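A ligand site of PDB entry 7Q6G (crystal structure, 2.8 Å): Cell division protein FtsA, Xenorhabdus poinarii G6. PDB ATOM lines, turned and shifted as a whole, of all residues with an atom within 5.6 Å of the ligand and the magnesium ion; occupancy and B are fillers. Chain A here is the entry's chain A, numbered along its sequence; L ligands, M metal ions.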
ATOM      1  N   GLU A  14     -42.652 -19.973 -21.572  1.00  0.00           N
ATOM      2  CA  GLU A  14     -41.273 -20.438 -21.504  1.00  0.00           C
ATOM      3  C   GLU A  14     -40.408 -19.300 -20.976  1.00  0.00           C
ATOM      4  O   GLU A  14     -40.343 -18.237 -21.594  1.00  0.00           O
ATOM      5  CB  GLU A  14     -40.774 -20.900 -22.874  1.00  0.00           C
ATOM      6  CG  GLU A  14     -39.423 -21.611 -22.840  1.00  0.00           C
ATOM      7  CD  GLU A  14     -38.890 -21.929 -24.223  1.00  0.00           C
ATOM      8  OE1 GLU A  14     -39.382 -21.338 -25.212  1.00  0.00           O
ATOM      9  OE2 GLU A  14     -37.964 -22.769 -24.334  1.00  0.00           O
ATOM     10  N   GLY A  16     -36.935 -18.623 -20.749  1.00  0.00           N
ATOM     11  CA  GLY A  16     -35.676 -19.106 -21.262  1.00  0.00           C
ATOM     12  C   GLY A  16     -34.485 -18.290 -20.786  1.00  0.00           C
ATOM     13  O   GLY A  16     -34.591 -17.425 -19.913  1.00  0.00           O
ATOM     14  N   THR A  17     -33.332 -18.576 -21.396  1.00  0.00           N
ATOM     15  CA  THR A  17     -32.091 -17.902 -21.014  1.00  0.00           C
ATOM     16  C   THR A  17     -32.005 -16.495 -21.580  1.00  0.00           C
ATOM     17  O   THR A  17     -31.380 -15.625 -20.960  1.00  0.00           O
ATOM     18  CB  THR A  17     -30.889 -18.726 -21.472  1.00  0.00           C
ATOM     19  OG1 THR A  17     -30.869 -18.796 -22.906  1.00  0.00           O
ATOM     20  CG2 THR A  17     -30.965 -20.143 -20.916  1.00  0.00           C
ATOM     21  N   ALA A  18     -32.611 -16.246 -22.738  1.00  0.00           N
ATOM     22  CA  ALA A  18     -32.607 -14.926 -23.351  1.00  0.00           C
ATOM     23  C   ALA A  18     -33.987 -14.381 -23.676  1.00  0.00           C
ATOM     24  O   ALA A  18     -34.132 -13.160 -23.826  1.00  0.00           O
ATOM     25  CB  ALA A  18     -31.757 -14.921 -24.633  1.00  0.00           C
ATOM     26  N   LYS A  19     -35.007 -15.231 -23.816  1.00  0.00           N
ATOM     27  CA  LYS A  19     -36.359 -14.795 -24.159  1.00  0.00           C
ATOM     28  C   LYS A  19     -37.352 -15.392 -23.179  1.00  0.00           C
ATOM     29  O   LYS A  19     -37.199 -16.534 -22.734  1.00  0.00           O
ATOM     30  CB  LYS A  19     -36.737 -15.204 -25.592  1.00  0.00           C
ATOM     31  CG  LYS A  19     -35.599 -15.134 -26.595  1.00  0.00           C
ATOM     32  CD  LYS A  19     -35.530 -13.779 -27.276  1.00  0.00           C
ATOM     33  CE  LYS A  19     -34.332 -13.678 -28.203  1.00  0.00           C
ATOM     34  NZ  LYS A  19     -34.182 -12.313 -28.772  1.00  0.00           N
ATOM     35  N   SER A  84     -36.480 -26.490 -18.240  1.00  0.00           N
ATOM     36  CA  SER A  84     -35.203 -27.020 -18.702  1.00  0.00           C
ATOM     37  C   SER A  84     -34.218 -27.003 -17.546  1.00  0.00           C
ATOM     38  O   SER A  84     -34.471 -26.451 -16.478  1.00  0.00           O
ATOM     39  CB  SER A  84     -34.631 -26.218 -19.875  1.00  0.00           C
ATOM     40  OG  SER A  84     -35.641 -25.783 -20.759  1.00  0.00           O
ATOM     41  N   ASP A 210     -33.403 -30.892 -29.138  1.00  0.00           N
ATOM     42  CA  ASP A 210     -33.734 -29.502 -28.851  1.00  0.00           C
ATOM     43  C   ASP A 210     -32.475 -28.783 -28.397  1.00  0.00           C
ATOM     44  O   ASP A 210     -31.992 -29.019 -27.282  1.00  0.00           O
ATOM     45  CB  ASP A 210     -34.847 -29.418 -27.797  1.00  0.00           C
ATOM     46  CG  ASP A 210     -35.390 -28.010 -27.626  1.00  0.00           C
ATOM     47  OD1 ASP A 210     -35.585 -27.316 -28.654  1.00  0.00           O
ATOM     48  OD2 ASP A 210     -35.624 -27.601 -26.475  1.00  0.00           O
ATOM     49  N   ILE A 211     -31.934 -27.929 -29.251  1.00  0.00           N
ATOM     50  CA  ILE A 211     -30.661 -27.268 -29.010  1.00  0.00           C
ATOM     51  C   ILE A 211     -30.958 -25.844 -28.561  1.00  0.00           C
ATOM     52  O   ILE A 211     -31.302 -24.980 -29.365  1.00  0.00           O
ATOM     53  CB  ILE A 211     -29.760 -27.295 -30.248  1.00  0.00           C
ATOM     54  CG1 ILE A 211     -29.772 -28.687 -30.876  1.00  0.00           C
ATOM     55  CG2 ILE A 211     -28.348 -26.876 -29.887  1.00  0.00           C
ATOM     56  CD1 ILE A 211     -28.742 -28.883 -31.961  1.00  0.00           C
ATOM     57  N   GLY A 212     -30.820 -25.592 -27.265  1.00  0.00           N
ATOM     58  CA  GLY A 212     -30.998 -24.283 -26.691  1.00  0.00           C
ATOM     59  C   GLY A 212     -29.688 -23.541 -26.524  1.00  0.00           C
ATOM     60  O   GLY A 212     -28.753 -23.707 -27.311  1.00  0.00           O
ATOM     61  N   GLY A 213     -29.612 -22.725 -25.476  1.00  0.00           N
ATOM     62  CA  GLY A 213     -28.396 -22.009 -25.167  1.00  0.00           C
ATOM     63  C   GLY A 213     -27.448 -22.802 -24.307  1.00  0.00           C
ATOM     64  O   GLY A 213     -26.242 -22.850 -24.578  1.00  0.00           O
ATOM     65  N   GLY A 214     -27.975 -23.453 -23.269  1.00  0.00           N
ATOM     66  CA  GLY A 214     -27.134 -24.160 -22.331  1.00  0.00           C
ATOM     67  C   GLY A 214     -27.320 -25.667 -22.306  1.00  0.00           C
ATOM     68  O   GLY A 214     -26.462 -26.389 -21.793  1.00  0.00           O
ATOM     69  N   THR A 215     -28.422 -26.158 -22.870  1.00  0.00           N
ATOM     70  CA  THR A 215     -28.721 -27.579 -22.866  1.00  0.00           C
ATOM     71  C   THR A 215     -29.068 -28.060 -24.260  1.00  0.00           C
ATOM     72  O   THR A 215     -29.556 -27.301 -25.101  1.00  0.00           O
ATOM     73  CB  THR A 215     -29.873 -27.918 -21.909  1.00  0.00           C
ATOM     74  OG1 THR A 215     -30.976 -27.023 -22.142  1.00  0.00           O
ATOM     75  CG2 THR A 215     -29.438 -27.808 -20.460  1.00  0.00           C
ATOM     76  N   GLY A 236     -25.377 -23.908 -27.603  1.00  0.00           N
ATOM     77  CA  GLY A 236     -24.947 -22.720 -28.330  1.00  0.00           C
ATOM     78  C   GLY A 236     -24.088 -21.759 -27.536  1.00  0.00           C
ATOM     79  O   GLY A 236     -23.431 -20.909 -28.145  1.00  0.00           O
ATOM     80  N   ASN A 237     -24.089 -21.852 -26.201  1.00  0.00           N
ATOM     81  CA  ASN A 237     -23.255 -20.965 -25.402  1.00  0.00           C
ATOM     82  C   ASN A 237     -21.790 -21.392 -25.436  1.00  0.00           C
ATOM     83  O   ASN A 237     -20.907 -20.525 -25.390  1.00  0.00           O
ATOM     84  CB  ASN A 237     -23.755 -20.915 -23.956  1.00  0.00           C
ATOM     85  CG  ASN A 237     -25.033 -20.097 -23.808  1.00  0.00           C
ATOM     86  OD1 ASN A 237     -25.517 -19.501 -24.774  1.00  0.00           O
ATOM     87  ND2 ASN A 237     -25.575 -20.085 -22.601  1.00  0.00           N
ATOM     88  N   THR A 240     -20.479 -20.067 -28.657  1.00  0.00           N
ATOM     89  CA  THR A 240     -20.215 -18.640 -28.525  1.00  0.00           C
ATOM     90  C   THR A 240     -18.922 -18.378 -27.752  1.00  0.00           C
ATOM     91  O   THR A 240     -18.199 -17.422 -28.050  1.00  0.00           O
ATOM     92  CB  THR A 240     -21.383 -17.950 -27.830  1.00  0.00           C
ATOM     93  OG1 THR A 240     -22.609 -18.335 -28.471  1.00  0.00           O
ATOM     94  CG2 THR A 240     -21.241 -16.439 -27.903  1.00  0.00           C
ATOM     95  N   GLU A 255     -21.558 -13.407 -29.551  1.00  0.00           N
ATOM     96  CA  GLU A 255     -22.922 -13.875 -29.755  1.00  0.00           C
ATOM     97  C   GLU A 255     -23.552 -13.217 -30.970  1.00  0.00           C
ATOM     98  O   GLU A 255     -24.284 -13.869 -31.732  1.00  0.00           O
ATOM     99  CB  GLU A 255     -23.759 -13.591 -28.503  1.00  0.00           C
ATOM    100  CG  GLU A 255     -25.244 -13.877 -28.658  1.00  0.00           C
ATOM    101  CD  GLU A 255     -25.574 -15.347 -28.537  1.00  0.00           C
ATOM    102  OE1 GLU A 255     -24.795 -16.094 -27.909  1.00  0.00           O
ATOM    103  OE2 GLU A 255     -26.620 -15.761 -29.078  1.00  0.00           O
ATOM    104  N   LYS A 258     -22.106 -14.701 -34.280  1.00  0.00           N
ATOM    105  CA  LYS A 258     -22.523 -16.085 -34.512  1.00  0.00           C
ATOM    106  C   LYS A 258     -23.908 -16.136 -35.133  1.00  0.00           C
ATOM    107  O   LYS A 258     -24.129 -16.843 -36.126  1.00  0.00           O
ATOM    108  CB  LYS A 258     -22.493 -16.873 -33.210  1.00  0.00           C
ATOM    109  CG  LYS A 258     -22.746 -18.369 -33.400  1.00  0.00           C
ATOM    110  CD  LYS A 258     -22.888 -19.075 -32.062  1.00  0.00           C
ATOM    111  CE  LYS A 258     -24.174 -18.665 -31.369  1.00  0.00           C
ATOM    112  NZ  LYS A 258     -24.277 -19.226 -29.997  1.00  0.00           N
ATOM    113  N   VAL A 259     -24.865 -15.393 -34.567  1.00  0.00           N
ATOM    114  CA  VAL A 259     -26.213 -15.401 -35.128  1.00  0.00           C
ATOM    115  C   VAL A 259     -26.254 -14.676 -36.463  1.00  0.00           C
ATOM    116  O   VAL A 259     -27.013 -15.048 -37.359  1.00  0.00           O
ATOM    117  CB  VAL A 259     -27.199 -14.775 -34.116  1.00  0.00           C
ATOM    118  CG1 VAL A 259     -28.633 -14.871 -34.632  1.00  0.00           C
ATOM    119  CG2 VAL A 259     -27.070 -15.473 -32.765  1.00  0.00           C
ATOM    120  N   TYR A 301     -19.604 -27.770 -33.047  1.00  0.00           N
ATOM    121  CA  TYR A 301     -20.903 -28.316 -33.402  1.00  0.00           C
ATOM    122  C   TYR A 301     -20.807 -29.804 -33.732  1.00  0.00           C
ATOM    123  O   TYR A 301     -21.680 -30.591 -33.348  1.00  0.00           O
ATOM    124  CB  TYR A 301     -21.499 -27.545 -34.574  1.00  0.00           C
ATOM    125  CG  TYR A 301     -22.630 -26.612 -34.178  1.00  0.00           C
ATOM    126  CD1 TYR A 301     -23.930 -27.080 -34.057  1.00  0.00           C
ATOM    127  CD2 TYR A 301     -22.389 -25.266 -33.945  1.00  0.00           C
ATOM    128  CE1 TYR A 301     -24.961 -26.228 -33.690  1.00  0.00           C
ATOM    129  CE2 TYR A 301     -23.407 -24.408 -33.592  1.00  0.00           C
ATOM    130  CZ  TYR A 301     -24.697 -24.897 -33.470  1.00  0.00           C
ATOM    131  OH  TYR A 301     -25.709 -24.045 -33.114  1.00  0.00           O
ATOM    132  N   GLY A 336     -34.853 -26.087 -31.826  1.00  0.00           N
ATOM    133  CA  GLY A 336     -34.381 -25.121 -30.852  1.00  0.00           C
ATOM    134  C   GLY A 336     -33.706 -23.940 -31.512  1.00  0.00           C
ATOM    135  O   GLY A 336     -33.521 -23.879 -32.731  1.00  0.00           O
ATOM    136  N   GLY A 337     -33.333 -22.971 -30.672  1.00  0.00           N
ATOM    137  CA  GLY A 337     -32.655 -21.798 -31.184  1.00  0.00           C
ATOM    138  C   GLY A 337     -31.300 -22.119 -31.773  1.00  0.00           C
ATOM    139  O   GLY A 337     -30.936 -21.601 -32.834  1.00  0.00           O
ATOM    140  N   GLY A 338     -30.527 -22.971 -31.094  1.00  0.00           N
ATOM    141  CA  GLY A 338     -29.214 -23.342 -31.575  1.00  0.00           C
ATOM    142  C   GLY A 338     -29.204 -24.157 -32.849  1.00  0.00           C
ATOM    143  O   GLY A 338     -28.121 -24.415 -33.384  1.00  0.00           O
ATOM    144  N   ALA A 339     -30.370 -24.566 -33.340  1.00  0.00           N
ATOM    145  CA  ALA A 339     -30.458 -25.349 -34.562  1.00  0.00           C
ATOM    146  C   ALA A 339     -30.659 -24.495 -35.807  1.00  0.00           C
ATOM    147  O   ALA A 339     -30.703 -25.034 -36.914  1.00  0.00           O
ATOM    148  CB  ALA A 339     -31.598 -26.367 -34.446  1.00  0.00           C
ATOM    149  N   GLN A 340     -30.773 -23.176 -35.650  1.00  0.00           N
ATOM    150  CA  GLN A 340     -31.054 -22.274 -36.767  1.00  0.00           C
ATOM    151  C   GLN A 340     -29.810 -21.821 -37.510  1.00  0.00           C
ATOM    152  O   GLN A 340     -29.929 -21.073 -38.481  1.00  0.00           O
ATOM    153  CB  GLN A 340     -31.819 -21.053 -36.255  1.00  0.00           C
ATOM    154  CG  GLN A 340     -33.259 -21.334 -35.869  1.00  0.00           C
ATOM    155  CD  GLN A 340     -33.852 -20.265 -34.973  1.00  0.00           C
ATOM    156  OE1 GLN A 340     -35.051 -20.005 -34.995  1.00  0.00           O
ATOM    157  NE2 GLN A 340     -32.994 -19.639 -34.169  1.00  0.00           N
ATOM    158  N   ILE A 341     -28.619 -22.267 -37.089  1.00  0.00           N
ATOM    159  CA  ILE A 341     -27.397 -21.840 -37.752  1.00  0.00           C
ATOM    160  C   ILE A 341     -27.331 -22.452 -39.148  1.00  0.00           C
ATOM    161  O   ILE A 341     -27.862 -23.543 -39.405  1.00  0.00           O
ATOM    162  CB  ILE A 341     -26.157 -22.216 -36.911  1.00  0.00           C
ATOM    163  CG1 ILE A 341     -24.902 -21.547 -37.469  1.00  0.00           C
ATOM    164  CG2 ILE A 341     -25.976 -23.724 -36.852  1.00  0.00           C
ATOM    165  CD1 ILE A 341     -23.834 -21.291 -36.426  1.00  0.00           C
ATOM    166  N   ASP A 342     -26.681 -21.744 -40.074  1.00  0.00           N
ATOM    167  CA  ASP A 342     -26.511 -22.233 -41.432  1.00  0.00           C
ATOM    168  C   ASP A 342     -25.726 -23.540 -41.430  1.00  0.00           C
ATOM    169  O   ASP A 342     -24.941 -23.823 -40.514  1.00  0.00           O
ATOM    170  CB  ASP A 342     -25.769 -21.196 -42.280  1.00  0.00           C
ATOM    171  CG  ASP A 342     -26.686 -20.099 -42.783  1.00  0.00           C
ATOM    172  OD1 ASP A 342     -27.848 -20.025 -42.329  1.00  0.00           O
ATOM    173  OD2 ASP A 342     -26.234 -19.298 -43.637  1.00  0.00           O
ATOM    174  N   CYS A 375     -36.770 -21.847 -32.771  1.00  0.00           N
ATOM    175  CA  CYS A 375     -36.610 -21.520 -31.360  1.00  0.00           C
ATOM    176  C   CYS A 375     -37.938 -21.545 -30.607  1.00  0.00           C
ATOM    177  O   CYS A 375     -37.938 -21.614 -29.372  1.00  0.00           O
ATOM    178  CB  CYS A 375     -35.947 -20.149 -31.213  1.00  0.00           C
ATOM    179  SG  CYS A 375     -36.980 -18.735 -31.667  1.00  0.00           S
ATOM    180  N   THR A 378     -40.401 -25.295 -28.176  1.00  0.00           N
ATOM    181  CA  THR A 378     -40.912 -25.577 -26.837  1.00  0.00           C
ATOM    182  C   THR A 378     -42.191 -24.796 -26.554  1.00  0.00           C
ATOM    183  O   THR A 378     -43.155 -25.352 -26.009  1.00  0.00           O
ATOM    184  CB  THR A 378     -39.839 -25.246 -25.789  1.00  0.00           C
ATOM    185  OG1 THR A 378     -38.633 -25.961 -26.094  1.00  0.00           O
ATOM    186  CG2 THR A 378     -40.325 -25.634 -24.401  1.00  0.00           C
HETATM  187  P1  LIG L   1     -33.229 -21.779 -24.508  1.00  0.00           P
HETATM  188  O1  LIG L   1     -34.108 -20.631 -24.092  1.00  0.00           O
HETATM  189  O2  LIG L   1     -33.976 -23.005 -24.997  1.00  0.00           O
HETATM  190  O3  LIG L   1     -32.097 -22.083 -23.554  1.00  0.00           O
HETATM  191  P2  LIG L   1     -33.203 -20.924 -27.217  1.00  0.00           P
HETATM  192  O4  LIG L   1     -33.852 -19.562 -27.112  1.00  0.00           O
HETATM  193  O5  LIG L   1     -34.017 -22.125 -27.644  1.00  0.00           O
HETATM  194  O6  LIG L   1     -32.464 -21.244 -25.824  1.00  0.00           O
HETATM  195  O7  LIG L   1     -31.902 -20.815 -28.164  1.00  0.00           O
HETATM  196  C1  LIG L   1     -30.943 -19.792 -27.913  1.00  0.00           C
HETATM  197  C2  LIG L   1     -29.603 -20.197 -28.506  1.00  0.00           C
HETATM  198  O8  LIG L   1     -29.724 -20.336 -29.921  1.00  0.00           O
HETATM  199  C3  LIG L   1     -28.547 -19.136 -28.241  1.00  0.00           C
HETATM  200  O9  LIG L   1     -27.378 -19.757 -27.688  1.00  0.00           O
HETATM  201  C4  LIG L   1     -28.202 -18.568 -29.599  1.00  0.00           C
HETATM  202  O10 LIG L   1     -26.801 -18.334 -29.709  1.00  0.00           O
HETATM  203  C5  LIG L   1     -28.663 -19.634 -30.574  1.00  0.00           C
HETATM  204  N1  LIG L   1     -29.133 -19.042 -31.856  1.00  0.00           N
HETATM  205  C6  LIG L   1     -30.270 -18.346 -32.057  1.00  0.00           C
HETATM  206  N2  LIG L   1     -30.377 -17.947 -33.353  1.00  0.00           N
HETATM  207  C7  LIG L   1     -29.285 -18.390 -34.003  1.00  0.00           C
HETATM  208  C8  LIG L   1     -28.753 -18.323 -35.392  1.00  0.00           C
HETATM  209  N3  LIG L   1     -29.435 -17.686 -36.374  1.00  0.00           N
HETATM  210  N4  LIG L   1     -27.569 -18.919 -35.644  1.00  0.00           N
HETATM  211  C9  LIG L   1     -26.878 -19.558 -34.683  1.00  0.00           C
HETATM  212  N5  LIG L   1     -27.299 -19.660 -33.405  1.00  0.00           N
HETATM  213  C10 LIG L   1     -28.466 -19.106 -33.006  1.00  0.00           C
HETATM  214 MG    MG M   1     -35.236 -23.724 -26.945  1.00  0.00          MG
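The magnesium ion is bound by an oxygen (O5) of the ligand (2.1 Å) and an oxygen (O2) of the ligand (2.4 Å).
The side-chain carboxylate (OE2) of Glu 255 lies within hydrogen-bond range of an oxygen (O10) of the ligand (2.7 Å). O10 of the ligand sits at hydrogen-bond distance from NZ of Lys 258, at 2.7 Å. N of Thr 17 lies within hydrogen-bond range of O1 of the ligand, at 3.5 Å. N of Gly 337 sits close to O5 of the ligand, 3.2 Å away. O9 of the ligand is in hydrogen-bond range of OD1 of Asn 237 (3.5 Å). An oxygen (O3) of the ligand lies within hydrogen-bond range of the backbone NH (N) of Gly 213, 3.2 Å away. An oxygen (O8) of the ligand sits at hydrogen-bond distance from the backbone NH of Gly 338 (3.0 Å). The side-chain amide nitrogen of Gln 340 lies within hydrogen-bond range of a nitrogen (N2) of the ligand (3.2 Å).
Gly 16 touches the ligand. Gly 212 touches the ligand. C of Gly 236 touches O9 of the ligand, at 3.9 Å. CG1 of Val 259 touches N3 of the ligand, 3.4 Å away. CB of Ile 341 touches C9 of the ligand, at 3.5 Å. Hydrophobic or aromatic side chains within 4 Å of the ligand: Val 259 and Ile 341.
The side-chain carboxylate of Glu 255 sits at hydrogen-bond distance from the side-chain hydroxyl of Thr 240 (3.2 Å). The backbone NH (N) of Gly 338 is in hydrogen-bond range of the backbone carbonyl oxygen (O) of Ile 211 (2.8 Å). The backbone NH (N) of Gly 236 is in hydrogen-bond range of the backbone carbonyl oxygen (O) of Gly 213 (3.3 Å). The side-chain carboxylate of Asp 210 lies within hydrogen-bond range of the side-chain hydroxyl of Thr 378 (3.4 Å). NZ of Lys 258 is in hydrogen-bond range of OG1 of Thr 240, at 2.4 Å. The backbone NH (N) of Cys 375 lies within hydrogen-bond range of the side-chain amide oxygen (OE1) of Gln 340 (3.4 Å). The side-chain hydroxyl of Tyr 301 is in hydrogen-bond range of the backbone carbonyl oxygen of Gly 338. The side-chain carboxylate of Asp 210 lies close to the backbone NH of Gly 336.
Merely in contact with the magnesium ion: Glu 14 and Asp 210. Of the 28 residues printed, 2 come within 4 Å of the magnesium ion. Along chain A the residues within 4 Å of the magnesium ion span positions 14 to 210.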
